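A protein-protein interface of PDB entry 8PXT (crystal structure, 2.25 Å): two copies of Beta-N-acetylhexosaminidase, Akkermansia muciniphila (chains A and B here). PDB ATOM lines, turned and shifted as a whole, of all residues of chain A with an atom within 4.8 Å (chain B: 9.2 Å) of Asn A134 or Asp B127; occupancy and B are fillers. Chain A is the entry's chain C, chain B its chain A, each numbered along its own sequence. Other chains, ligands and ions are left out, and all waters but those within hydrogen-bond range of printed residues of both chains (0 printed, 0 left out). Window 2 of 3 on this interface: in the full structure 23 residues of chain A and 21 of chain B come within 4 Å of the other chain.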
ATOM      1  N   SER A  18      21.209 -15.057 -32.006  1.00  0.00           N
ATOM      2  CA  SER A  18      20.621 -13.955 -31.268  1.00  0.00           C
ATOM      3  C   SER A  18      19.572 -14.461 -30.290  1.00  0.00           C
ATOM      4  O   SER A  18      18.981 -15.529 -30.480  1.00  0.00           O
ATOM      5  CB  SER A  18      19.996 -12.945 -32.234  1.00  0.00           C
ATOM      6  OG  SER A  18      19.076 -13.577 -33.101  1.00  0.00           O
ATOM      7  N   PRO A  19      19.312 -13.710 -29.227  1.00  0.00           N
ATOM      8  CA  PRO A  19      18.450 -14.212 -28.159  1.00  0.00           C
ATOM      9  C   PRO A  19      16.975 -13.993 -28.457  1.00  0.00           C
ATOM     10  O   PRO A  19      16.592 -13.211 -29.329  1.00  0.00           O
ATOM     11  CB  PRO A  19      18.896 -13.390 -26.945  1.00  0.00           C
ATOM     12  CG  PRO A  19      19.341 -12.080 -27.535  1.00  0.00           C
ATOM     13  CD  PRO A  19      19.788 -12.341 -28.958  1.00  0.00           C
ATOM     14  N   ALA A  20      16.144 -14.725 -27.720  1.00  0.00           N
ATOM     15  CA  ALA A  20      14.720 -14.433 -27.702  1.00  0.00           C
ATOM     16  C   ALA A  20      14.497 -13.034 -27.141  1.00  0.00           C
ATOM     17  O   ALA A  20      15.231 -12.570 -26.264  1.00  0.00           O
ATOM     18  CB  ALA A  20      13.972 -15.463 -26.856  1.00  0.00           C
ATOM     19  N   ARG A  21      13.477 -12.354 -27.657  1.00  0.00           N
ATOM     20  CA  ARG A  21      13.190 -10.987 -27.242  1.00  0.00           C
ATOM     21  C   ARG A  21      11.688 -10.787 -27.126  1.00  0.00           C
ATOM     22  O   ARG A  21      10.945 -11.070 -28.069  1.00  0.00           O
ATOM     23  CB  ARG A  21      13.784  -9.971 -28.227  1.00  0.00           C
ATOM     24  CG  ARG A  21      13.530  -8.522 -27.830  1.00  0.00           C
ATOM     25  CD  ARG A  21      14.409  -7.538 -28.596  1.00  0.00           C
ATOM     26  NE  ARG A  21      14.024  -7.400 -29.996  1.00  0.00           N
ATOM     27  CZ  ARG A  21      13.033  -6.633 -30.431  1.00  0.00           C
ATOM     28  NH1 ARG A  21      12.266  -5.953 -29.594  1.00  0.00           N
ATOM     29  NH2 ARG A  21      12.803  -6.549 -31.739  1.00  0.00           N
ATOM     30  N   MET A 116      17.670 -12.914 -16.378  1.00  0.00           N
ATOM     31  CA  MET A 116      18.264 -12.902 -17.707  1.00  0.00           C
ATOM     32  C   MET A 116      17.789 -11.721 -18.550  1.00  0.00           C
ATOM     33  O   MET A 116      18.089 -11.667 -19.746  1.00  0.00           O
ATOM     34  CB  MET A 116      17.966 -14.223 -18.423  1.00  0.00           C
ATOM     35  CG  MET A 116      18.645 -15.429 -17.776  1.00  0.00           C
ATOM     36  SD  MET A 116      18.595 -16.929 -18.780  1.00  0.00           S
ATOM     37  CE  MET A 116      16.902 -17.456 -18.535  1.00  0.00           C
ATOM     38  N   MET A 117      17.073 -10.772 -17.952  1.00  0.00           N
ATOM     39  CA  MET A 117      16.576  -9.585 -18.627  1.00  0.00           C
ATOM     40  C   MET A 117      17.153  -8.330 -17.982  1.00  0.00           C
ATOM     41  O   MET A 117      17.632  -8.369 -16.841  1.00  0.00           O
ATOM     42  CB  MET A 117      15.040  -9.521 -18.578  1.00  0.00           C
ATOM     43  CG  MET A 117      14.338 -10.624 -19.364  1.00  0.00           C
ATOM     44  SD  MET A 117      12.552 -10.388 -19.484  1.00  0.00           S
ATOM     45  CE  MET A 117      12.073 -10.531 -17.768  1.00  0.00           C
ATOM     46  N   PRO A 118      17.120  -7.197 -18.684  1.00  0.00           N
ATOM     47  CA  PRO A 118      17.659  -5.953 -18.120  1.00  0.00           C
ATOM     48  C   PRO A 118      17.133  -5.679 -16.718  1.00  0.00           C
ATOM     49  O   PRO A 118      15.966  -5.926 -16.409  1.00  0.00           O
ATOM     50  CB  PRO A 118      17.191  -4.892 -19.120  1.00  0.00           C
ATOM     51  CG  PRO A 118      17.150  -5.630 -20.419  1.00  0.00           C
ATOM     52  CD  PRO A 118      16.675  -7.017 -20.079  1.00  0.00           C
ATOM     53  N   ARG A 132      15.413  -3.117 -24.581  1.00  0.00           N
ATOM     54  CA  ARG A 132      15.257  -4.305 -25.417  1.00  0.00           C
ATOM     55  C   ARG A 132      15.169  -5.512 -24.486  1.00  0.00           C
ATOM     56  O   ARG A 132      16.149  -5.863 -23.821  1.00  0.00           O
ATOM     57  CB  ARG A 132      16.420  -4.447 -26.395  1.00  0.00           C
ATOM     58  CG  ARG A 132      16.670  -3.231 -27.286  1.00  0.00           C
ATOM     59  CD  ARG A 132      15.820  -3.253 -28.545  1.00  0.00           C
ATOM     60  NE  ARG A 132      16.231  -4.295 -29.479  1.00  0.00           N
ATOM     61  CZ  ARG A 132      15.690  -4.484 -30.676  1.00  0.00           C
ATOM     62  NH1 ARG A 132      14.706  -3.719 -31.119  1.00  0.00           N
ATOM     63  NH2 ARG A 132      16.149  -5.464 -31.446  1.00  0.00           N
ATOM     64  N   TRP A 133      14.003  -6.152 -24.438  1.00  0.00           N
ATOM     65  CA  TRP A 133      13.742  -7.193 -23.442  1.00  0.00           C
ATOM     66  C   TRP A 133      14.230  -8.549 -23.956  1.00  0.00           C
ATOM     67  O   TRP A 133      13.468  -9.481 -24.220  1.00  0.00           O
ATOM     68  CB  TRP A 133      12.263  -7.199 -23.078  1.00  0.00           C
ATOM     69  CG  TRP A 133      11.888  -5.949 -22.343  1.00  0.00           C
ATOM     70  CD1 TRP A 133      11.228  -4.863 -22.841  1.00  0.00           C
ATOM     71  CD2 TRP A 133      12.191  -5.645 -20.978  1.00  0.00           C
ATOM     72  NE1 TRP A 133      11.089  -3.905 -21.864  1.00  0.00           N
ATOM     73  CE2 TRP A 133      11.672  -4.363 -20.711  1.00  0.00           C
ATOM     74  CE3 TRP A 133      12.847  -6.334 -19.956  1.00  0.00           C
ATOM     75  CZ2 TRP A 133      11.791  -3.758 -19.464  1.00  0.00           C
ATOM     76  CZ3 TRP A 133      12.959  -5.734 -18.719  1.00  0.00           C
ATOM     77  CH2 TRP A 133      12.436  -4.460 -18.483  1.00  0.00           C
ATOM     78  N   ASN A 134      15.554  -8.643 -24.077  1.00  0.00           N
ATOM     79  CA  ASN A 134      16.206  -9.873 -24.500  1.00  0.00           C
ATOM     80  C   ASN A 134      16.339 -10.843 -23.333  1.00  0.00           C
ATOM     81  O   ASN A 134      16.626 -10.440 -22.202  1.00  0.00           O
ATOM     82  CB  ASN A 134      17.593  -9.565 -25.069  1.00  0.00           C
ATOM     83  CG  ASN A 134      17.536  -8.827 -26.389  1.00  0.00           C
ATOM     84  OD1 ASN A 134      16.923  -9.293 -27.347  1.00  0.00           O
ATOM     85  ND2 ASN A 134      18.178  -7.665 -26.446  1.00  0.00           N
ATOM     86  N   ILE A 135      16.132 -12.129 -23.614  1.00  0.00           N
ATOM     87  CA  ILE A 135      16.368 -13.191 -22.640  1.00  0.00           C
ATOM     88  C   ILE A 135      17.816 -13.636 -22.829  1.00  0.00           C
ATOM     89  O   ILE A 135      18.122 -14.446 -23.707  1.00  0.00           O
ATOM     90  CB  ILE A 135      15.398 -14.363 -22.810  1.00  0.00           C
ATOM     91  CG1 ILE A 135      13.947 -13.882 -22.946  1.00  0.00           C
ATOM     92  CG2 ILE A 135      15.530 -15.322 -21.628  1.00  0.00           C
ATOM     93  CD1 ILE A 135      13.438 -13.076 -21.777  1.00  0.00           C
ATOM     94  N   SER A 136      18.714 -13.102 -22.003  1.00  0.00           N
ATOM     95  CA  SER A 136      20.135 -13.396 -22.142  1.00  0.00           C
ATOM     96  C   SER A 136      20.628 -12.888 -23.494  1.00  0.00           C
ATOM     97  O   SER A 136      20.014 -11.993 -24.084  1.00  0.00           O
ATOM     98  CB  SER A 136      20.391 -14.896 -21.990  1.00  0.00           C
ATOM     99  OG  SER A 136      21.735 -15.148 -21.628  1.00  0.00           O
ATOM    100  N   GLY B  51      26.219 -11.318 -41.083  1.00  0.00           N
ATOM    101  CA  GLY B  51      26.834 -10.481 -40.068  1.00  0.00           C
ATOM    102  C   GLY B  51      25.920  -9.416 -39.505  1.00  0.00           C
ATOM    103  O   GLY B  51      26.016  -9.084 -38.318  1.00  0.00           O
ATOM    104  N   THR B  52      25.026  -8.865 -40.331  1.00  0.00           N
ATOM    105  CA  THR B  52      24.137  -7.801 -39.880  1.00  0.00           C
ATOM    106  C   THR B  52      22.799  -8.318 -39.376  1.00  0.00           C
ATOM    107  O   THR B  52      22.189  -7.684 -38.509  1.00  0.00           O
ATOM    108  CB  THR B  52      23.868  -6.798 -41.009  1.00  0.00           C
ATOM    109  OG1 THR B  52      23.211  -7.459 -42.101  1.00  0.00           O
ATOM    110  CG2 THR B  52      25.159  -6.168 -41.493  1.00  0.00           C
ATOM    111  N   GLY B  53      22.332  -9.455 -39.892  1.00  0.00           N
ATOM    112  CA  GLY B  53      20.982  -9.910 -39.651  1.00  0.00           C
ATOM    113  C   GLY B  53      19.960  -9.347 -40.611  1.00  0.00           C
ATOM    114  O   GLY B  53      18.834  -9.859 -40.666  1.00  0.00           O
ATOM    115  N   VAL B 120      30.659  -5.045 -34.290  1.00  0.00           N
ATOM    116  CA  VAL B 120      29.761  -6.099 -33.824  1.00  0.00           C
ATOM    117  C   VAL B 120      29.293  -6.991 -34.970  1.00  0.00           C
ATOM    118  O   VAL B 120      28.766  -8.083 -34.729  1.00  0.00           O
ATOM    119  CB  VAL B 120      28.562  -5.483 -33.068  1.00  0.00           C
ATOM    120  CG1 VAL B 120      27.850  -4.442 -33.920  1.00  0.00           C
ATOM    121  CG2 VAL B 120      27.590  -6.570 -32.640  1.00  0.00           C
ATOM    122  N   ASP B 123      30.218 -10.467 -34.389  1.00  0.00           N
ATOM    123  CA  ASP B 123      29.786 -11.165 -33.186  1.00  0.00           C
ATOM    124  C   ASP B 123      28.893 -12.343 -33.553  1.00  0.00           C
ATOM    125  O   ASP B 123      27.916 -12.189 -34.290  1.00  0.00           O
ATOM    126  CB  ASP B 123      29.040 -10.213 -32.255  1.00  0.00           C
ATOM    127  CG  ASP B 123      29.040 -10.685 -30.813  1.00  0.00           C
ATOM    128  OD1 ASP B 123      29.114 -11.912 -30.582  1.00  0.00           O
ATOM    129  OD2 ASP B 123      28.969  -9.827 -29.910  1.00  0.00           O
ATOM    130  N   ARG B 124      29.230 -13.520 -33.032  1.00  0.00           N
ATOM    131  CA  ARG B 124      28.411 -14.708 -33.231  1.00  0.00           C
ATOM    132  C   ARG B 124      27.198 -14.744 -32.303  1.00  0.00           C
ATOM    133  O   ARG B 124      26.378 -15.660 -32.421  1.00  0.00           O
ATOM    134  CB  ARG B 124      29.266 -15.967 -33.033  1.00  0.00           C
ATOM    135  CG  ARG B 124      30.505 -16.037 -33.933  1.00  0.00           C
ATOM    136  CD  ARG B 124      31.321 -17.308 -33.688  1.00  0.00           C
ATOM    137  NE  ARG B 124      32.493 -17.392 -34.554  1.00  0.00           N
ATOM    138  CZ  ARG B 124      33.326 -18.426 -34.596  1.00  0.00           C
ATOM    139  NH1 ARG B 124      33.142 -19.495 -33.838  1.00  0.00           N
ATOM    140  NH2 ARG B 124      34.367 -18.386 -35.423  1.00  0.00           N
ATOM    141  N   THR B 125      27.054 -13.764 -31.409  1.00  0.00           N
ATOM    142  CA  THR B 125      25.963 -13.730 -30.446  1.00  0.00           C
ATOM    143  C   THR B 125      25.375 -12.327 -30.373  1.00  0.00           C
ATOM    144  O   THR B 125      25.979 -11.350 -30.824  1.00  0.00           O
ATOM    145  CB  THR B 125      26.430 -14.135 -29.039  1.00  0.00           C
ATOM    146  OG1 THR B 125      27.348 -13.152 -28.538  1.00  0.00           O
ATOM    147  CG2 THR B 125      27.113 -15.495 -29.055  1.00  0.00           C
ATOM    148  N   GLY B 126      24.185 -12.238 -29.790  1.00  0.00           N
ATOM    149  CA  GLY B 126      23.651 -10.973 -29.338  1.00  0.00           C
ATOM    150  C   GLY B 126      22.586 -10.406 -30.261  1.00  0.00           C
ATOM    151  O   GLY B 126      22.454 -10.784 -31.428  1.00  0.00           O
ATOM    152  N   ASP B 127      21.819  -9.466 -29.711  1.00  0.00           N
ATOM    153  CA  ASP B 127      20.771  -8.762 -30.444  1.00  0.00           C
ATOM    154  C   ASP B 127      21.398  -7.739 -31.385  1.00  0.00           C
ATOM    155  O   ASP B 127      21.871  -6.688 -30.940  1.00  0.00           O
ATOM    156  CB  ASP B 127      19.828  -8.084 -29.453  1.00  0.00           C
ATOM    157  CG  ASP B 127      18.725  -7.299 -30.132  1.00  0.00           C
ATOM    158  OD1 ASP B 127      18.453  -7.561 -31.323  1.00  0.00           O
ATOM    159  OD2 ASP B 127      18.129  -6.417 -29.476  1.00  0.00           O
ATOM    160  N   LYS B 128      21.408  -8.037 -32.683  1.00  0.00           N
ATOM    161  CA  LYS B 128      21.893  -7.105 -33.691  1.00  0.00           C
ATOM    162  C   LYS B 128      20.770  -6.315 -34.347  1.00  0.00           C
ATOM    163  O   LYS B 128      21.044  -5.440 -35.173  1.00  0.00           O
ATOM    164  CB  LYS B 128      22.682  -7.846 -34.772  1.00  0.00           C
ATOM    165  CG  LYS B 128      24.033  -8.354 -34.315  1.00  0.00           C
ATOM    166  CD  LYS B 128      24.759  -9.024 -35.461  1.00  0.00           C
ATOM    167  CE  LYS B 128      25.890  -9.906 -34.981  1.00  0.00           C
ATOM    168  NZ  LYS B 128      26.173 -10.972 -35.977  1.00  0.00           N
ATOM    169  N   SER B 129      19.514  -6.605 -34.005  1.00  0.00           N
ATOM    170  CA  SER B 129      18.391  -5.870 -34.568  1.00  0.00           C
ATOM    171  C   SER B 129      18.364  -4.409 -34.130  1.00  0.00           C
ATOM    172  O   SER B 129      17.560  -3.637 -34.664  1.00  0.00           O
ATOM    173  CB  SER B 129      17.080  -6.560 -34.178  1.00  0.00           C
ATOM    174  OG  SER B 129      16.913  -7.777 -34.886  1.00  0.00           O
ATOM    175  N   ALA B 130      19.220  -4.012 -33.186  1.00  0.00           N
ATOM    176  CA  ALA B 130      19.278  -2.640 -32.702  1.00  0.00           C
ATOM    177  C   ALA B 130      20.460  -1.855 -33.255  1.00  0.00           C
ATOM    178  O   ALA B 130      20.529  -0.640 -33.042  1.00  0.00           O
ATOM    179  CB  ALA B 130      19.346  -2.625 -31.170  1.00  0.00           C
ATOM    180  N   VAL B 131      21.384  -2.512 -33.958  1.00  0.00           N
ATOM    181  CA  VAL B 131      22.587  -1.838 -34.430  1.00  0.00           C
ATOM    182  C   VAL B 131      22.228  -0.843 -35.523  1.00  0.00           C
ATOM    183  O   VAL B 131      21.368  -1.108 -36.375  1.00  0.00           O
ATOM    184  CB  VAL B 131      23.609  -2.869 -34.940  1.00  0.00           C
ATOM    185  CG1 VAL B 131      24.888  -2.179 -35.396  1.00  0.00           C
ATOM    186  CG2 VAL B 131      23.909  -3.903 -33.869  1.00  0.00           C
ATOM    187  N   ARG B 132      22.885   0.316 -35.502  1.00  0.00           N
ATOM    188  CA  ARG B 132      22.844   1.265 -36.611  1.00  0.00           C
ATOM    189  C   ARG B 132      23.952   0.874 -37.584  1.00  0.00           C
ATOM    190  O   ARG B 132      25.135   1.075 -37.293  1.00  0.00           O
ATOM    191  CB  ARG B 132      23.039   2.700 -36.124  1.00  0.00           C
ATOM    192  CG  ARG B 132      22.285   3.065 -34.857  1.00  0.00           C
ATOM    193  CD  ARG B 132      20.784   3.077 -35.069  1.00  0.00           C
ATOM    194  NE  ARG B 132      20.349   4.184 -35.912  1.00  0.00           N
ATOM    195  CZ  ARG B 132      19.088   4.408 -36.256  1.00  0.00           C
ATOM    196  NH1 ARG B 132      18.111   3.610 -35.857  1.00  0.00           N
ATOM    197  NH2 ARG B 132      18.799   5.460 -37.017  1.00  0.00           N
ATOM    198  N   TRP B 133      23.575   0.316 -38.731  1.00  0.00           N
ATOM    199  CA  TRP B 133      24.550  -0.188 -39.700  1.00  0.00           C
ATOM    200  C   TRP B 133      25.017   0.933 -40.630  1.00  0.00           C
ATOM    201  O   TRP B 133      24.866   0.891 -41.852  1.00  0.00           O
ATOM    202  CB  TRP B 133      23.957  -1.363 -40.469  1.00  0.00           C
ATOM    203  CG  TRP B 133      23.708  -2.533 -39.572  1.00  0.00           C
ATOM    204  CD1 TRP B 133      22.500  -3.006 -39.151  1.00  0.00           C
ATOM    205  CD2 TRP B 133      24.701  -3.360 -38.956  1.00  0.00           C
ATOM    206  NE1 TRP B 133      22.680  -4.086 -38.320  1.00  0.00           N
ATOM    207  CE2 TRP B 133      24.022  -4.322 -38.184  1.00  0.00           C
ATOM    208  CE3 TRP B 133      26.099  -3.383 -38.986  1.00  0.00           C
ATOM    209  CZ2 TRP B 133      24.692  -5.296 -37.448  1.00  0.00           C
ATOM    210  CZ3 TRP B 133      26.763  -4.353 -38.256  1.00  0.00           C
ATOM    211  CH2 TRP B 133      26.060  -5.297 -37.499  1.00  0.00           C
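The guanidinium group (NE) of Arg A132 is in salt-bridge range of the side-chain carboxylate (OD2) of Asp B127, 2.8 Å away.
OD2 of Asp B127 lies within hydrogen-bond range of ND2 of Asn A134.
OD1 of Asp B127 is in hydrogen-bond range of N of Ser B129 (3.0 Å).
O of Gly B126 touches CB of Ser A18, at 3.4 Å.
Gly B126 touches Pro A19 (C to CD, 3.6 Å).
Pro A19 touches Asp B127.
OD2 of Asp B127 touches CD of Arg A21, 3.98 Å away.
Arg A132 touches Ser B129.
Arg A132 touches Ala B130 (NH2 to N, 3.8 Å).
Of chain B, only Asp B127 (3.3 Å) comes within 4 Å of Asn A134.
Printed residues of chain A within 4 Å of Asp B127: Pro A19 (3.6 Å), Arg A21 (3.98 Å), Arg A132 (2.8 Å) and Asn A134 (3.3 Å).
No residue of chain B comes within 4 Å of Ile A135.
Of the printed residues of chain B, Pro A19 touches Gly B126 (3.6 Å) and Asp B127 (3.6 Å).
Printed residues of chain B within 4 Å of Arg A132: Asp B127 (2.8 Å), Ser B129 (3.1 Å) and Ala B130 (3.8 Å).
Printed residues of chain A within 4 Å of Gly B126: Ser A18 and Pro A19.
The nearest residue of chain B that does not touch Asn A134 is Gly B126 (6.4 Å).
Of the 15 printed residues of chain B, 4 touch a printed residue of chain A.
Printed residues of chain B that touch a printed residue of chain A: Gly B126, Asp B127, Ser B129 and Ala B130.
Printed residues of chain A that touch a printed residue of chain B: Ser A18, Pro A19, Arg A21, Arg A132 and Asn A134.
Among the printed residues, 8 pairs touch across the chains.
Positions printed for both chains: 132 and 133.
Of the 8 pairs that touch across the chains among the printed residues, none has its exchanged pair printed and touching as well.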
